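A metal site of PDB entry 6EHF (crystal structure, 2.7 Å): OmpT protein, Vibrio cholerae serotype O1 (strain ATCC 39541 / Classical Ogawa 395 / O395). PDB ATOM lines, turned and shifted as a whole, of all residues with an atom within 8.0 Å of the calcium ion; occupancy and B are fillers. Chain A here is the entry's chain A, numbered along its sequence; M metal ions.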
ATOM      1  N   VAL A   5      16.395  17.615 -11.292  1.00  0.00           N
ATOM      2  CA  VAL A   5      17.341  18.566 -10.722  1.00  0.00           C
ATOM      3  C   VAL A   5      18.560  18.660 -11.658  1.00  0.00           C
ATOM      4  O   VAL A   5      19.372  17.753 -11.676  1.00  0.00           O
ATOM      5  CB  VAL A   5      17.738  18.215  -9.243  1.00  0.00           C
ATOM      6  CG1 VAL A   5      18.332  16.810  -9.069  1.00  0.00           C
ATOM      7  CG2 VAL A   5      18.681  19.249  -8.668  1.00  0.00           C
ATOM      8  N   ASP A   6      18.653  19.731 -12.476  1.00  0.00           N
ATOM      9  CA  ASP A   6      19.838  19.967 -13.337  1.00  0.00           C
ATOM     10  C   ASP A   6      20.846  21.016 -12.775  1.00  0.00           C
ATOM     11  O   ASP A   6      20.523  22.185 -12.644  1.00  0.00           O
ATOM     12  CB  ASP A   6      19.391  20.387 -14.747  1.00  0.00           C
ATOM     13  CG  ASP A   6      20.575  20.505 -15.732  1.00  0.00           C
ATOM     14  OD1 ASP A   6      21.676  19.949 -15.494  1.00  0.00           O
ATOM     15  OD2 ASP A   6      20.375  21.157 -16.781  1.00  0.00           O
ATOM     16  N   PHE A   7      22.064  20.566 -12.447  1.00  0.00           N
ATOM     17  CA  PHE A   7      23.184  21.429 -12.129  1.00  0.00           C
ATOM     18  C   PHE A   7      23.881  21.679 -13.462  1.00  0.00           C
ATOM     19  O   PHE A   7      24.353  20.734 -14.088  1.00  0.00           O
ATOM     20  CB  PHE A   7      24.100  20.772 -11.082  1.00  0.00           C
ATOM     21  CG  PHE A   7      25.449  21.484 -10.871  1.00  0.00           C
ATOM     22  CD1 PHE A   7      25.501  22.813 -10.466  1.00  0.00           C
ATOM     23  CD2 PHE A   7      26.665  20.815 -11.075  1.00  0.00           C
ATOM     24  CE1 PHE A   7      26.719  23.461 -10.293  1.00  0.00           C
ATOM     25  CE2 PHE A   7      27.885  21.456 -10.887  1.00  0.00           C
ATOM     26  CZ  PHE A   7      27.912  22.773 -10.492  1.00  0.00           C
ATOM     27  N   TYR A   8      23.931  22.955 -13.902  1.00  0.00           N
ATOM     28  CA  TYR A   8      24.439  23.397 -15.216  1.00  0.00           C
ATOM     29  C   TYR A   8      25.426  24.604 -15.119  1.00  0.00           C
ATOM     30  O   TYR A   8      25.562  25.253 -14.081  1.00  0.00           O
ATOM     31  CB  TYR A   8      23.260  23.740 -16.164  1.00  0.00           C
ATOM     32  CG  TYR A   8      22.559  25.026 -15.804  1.00  0.00           C
ATOM     33  CD1 TYR A   8      21.666  25.077 -14.735  1.00  0.00           C
ATOM     34  CD2 TYR A   8      22.833  26.213 -16.507  1.00  0.00           C
ATOM     35  CE1 TYR A   8      21.048  26.261 -14.366  1.00  0.00           C
ATOM     36  CE2 TYR A   8      22.209  27.417 -16.146  1.00  0.00           C
ATOM     37  CZ  TYR A   8      21.319  27.431 -15.072  1.00  0.00           C
ATOM     38  OH  TYR A   8      20.672  28.594 -14.684  1.00  0.00           O
ATOM     39  N   GLY A   9      26.110  24.891 -16.226  1.00  0.00           N
ATOM     40  CA  GLY A   9      27.023  25.984 -16.294  1.00  0.00           C
ATOM     41  C   GLY A   9      27.779  26.178 -17.578  1.00  0.00           C
ATOM     42  O   GLY A   9      27.667  25.399 -18.511  1.00  0.00           O
ATOM     43  N   GLY A  33      24.444  27.180 -12.368  1.00  0.00           N
ATOM     44  CA  GLY A  33      23.082  27.228 -11.848  1.00  0.00           C
ATOM     45  C   GLY A  33      22.499  25.894 -11.498  1.00  0.00           C
ATOM     46  O   GLY A  33      23.160  24.887 -11.566  1.00  0.00           O
ATOM     47  N   TYR A 318      30.677  23.823 -21.583  1.00  0.00           N
ATOM     48  CA  TYR A 318      29.321  23.727 -21.002  1.00  0.00           C
ATOM     49  C   TYR A 318      29.099  22.419 -20.205  1.00  0.00           C
ATOM     50  O   TYR A 318      29.748  21.388 -20.475  1.00  0.00           O
ATOM     51  CB  TYR A 318      28.289  23.690 -22.105  1.00  0.00           C
ATOM     52  CG  TYR A 318      28.150  24.893 -22.978  1.00  0.00           C
ATOM     53  CD1 TYR A 318      29.165  25.295 -23.824  1.00  0.00           C
ATOM     54  CD2 TYR A 318      26.942  25.574 -23.057  1.00  0.00           C
ATOM     55  CE1 TYR A 318      28.996  26.373 -24.694  1.00  0.00           C
ATOM     56  CE2 TYR A 318      26.765  26.654 -23.893  1.00  0.00           C
ATOM     57  CZ  TYR A 318      27.797  27.051 -24.717  1.00  0.00           C
ATOM     58  OH  TYR A 318      27.639  28.117 -25.562  1.00  0.00           O
ATOM     59  N   TRP A 319      28.131  22.463 -19.263  1.00  0.00           N
ATOM     60  CA  TRP A 319      27.717  21.284 -18.461  1.00  0.00           C
ATOM     61  C   TRP A 319      26.252  21.357 -17.962  1.00  0.00           C
ATOM     62  O   TRP A 319      25.459  22.214 -18.394  1.00  0.00           O
ATOM     63  CB  TRP A 319      28.673  21.022 -17.279  1.00  0.00           C
ATOM     64  CG  TRP A 319      28.581  21.966 -16.071  1.00  0.00           C
ATOM     65  CD1 TRP A 319      27.787  21.818 -14.995  1.00  0.00           C
ATOM     66  CD2 TRP A 319      29.335  23.158 -15.851  1.00  0.00           C
ATOM     67  NE1 TRP A 319      27.988  22.848 -14.108  1.00  0.00           N
ATOM     68  CE2 TRP A 319      28.940  23.688 -14.620  1.00  0.00           C
ATOM     69  CE3 TRP A 319      30.310  23.842 -16.600  1.00  0.00           C
ATOM     70  CZ2 TRP A 319      29.477  24.856 -14.105  1.00  0.00           C
ATOM     71  CZ3 TRP A 319      30.835  24.997 -16.097  1.00  0.00           C
ATOM     72  CH2 TRP A 319      30.423  25.486 -14.854  1.00  0.00           C
ATOM     73  OXT TRP A 319      25.840  20.538 -17.124  1.00  0.00           O
HETATM   74 CA    CA M   1      23.796  19.327 -16.256  1.00  0.00          CA
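The nearest printed residue that does not touch the calcium ion is Tyr 8 (4.2 Å).
The calcium ion is bound by OD1 of Asp 6, OXT of Trp 319 and O of Phe 7.
The backbone NH (N) of Trp 319 is in hydrogen-bond range of the backbone carbonyl oxygen (O) of Gly 9.
NE1 of Trp 319 sits close to O of Tyr 8, 3.4 Å away.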
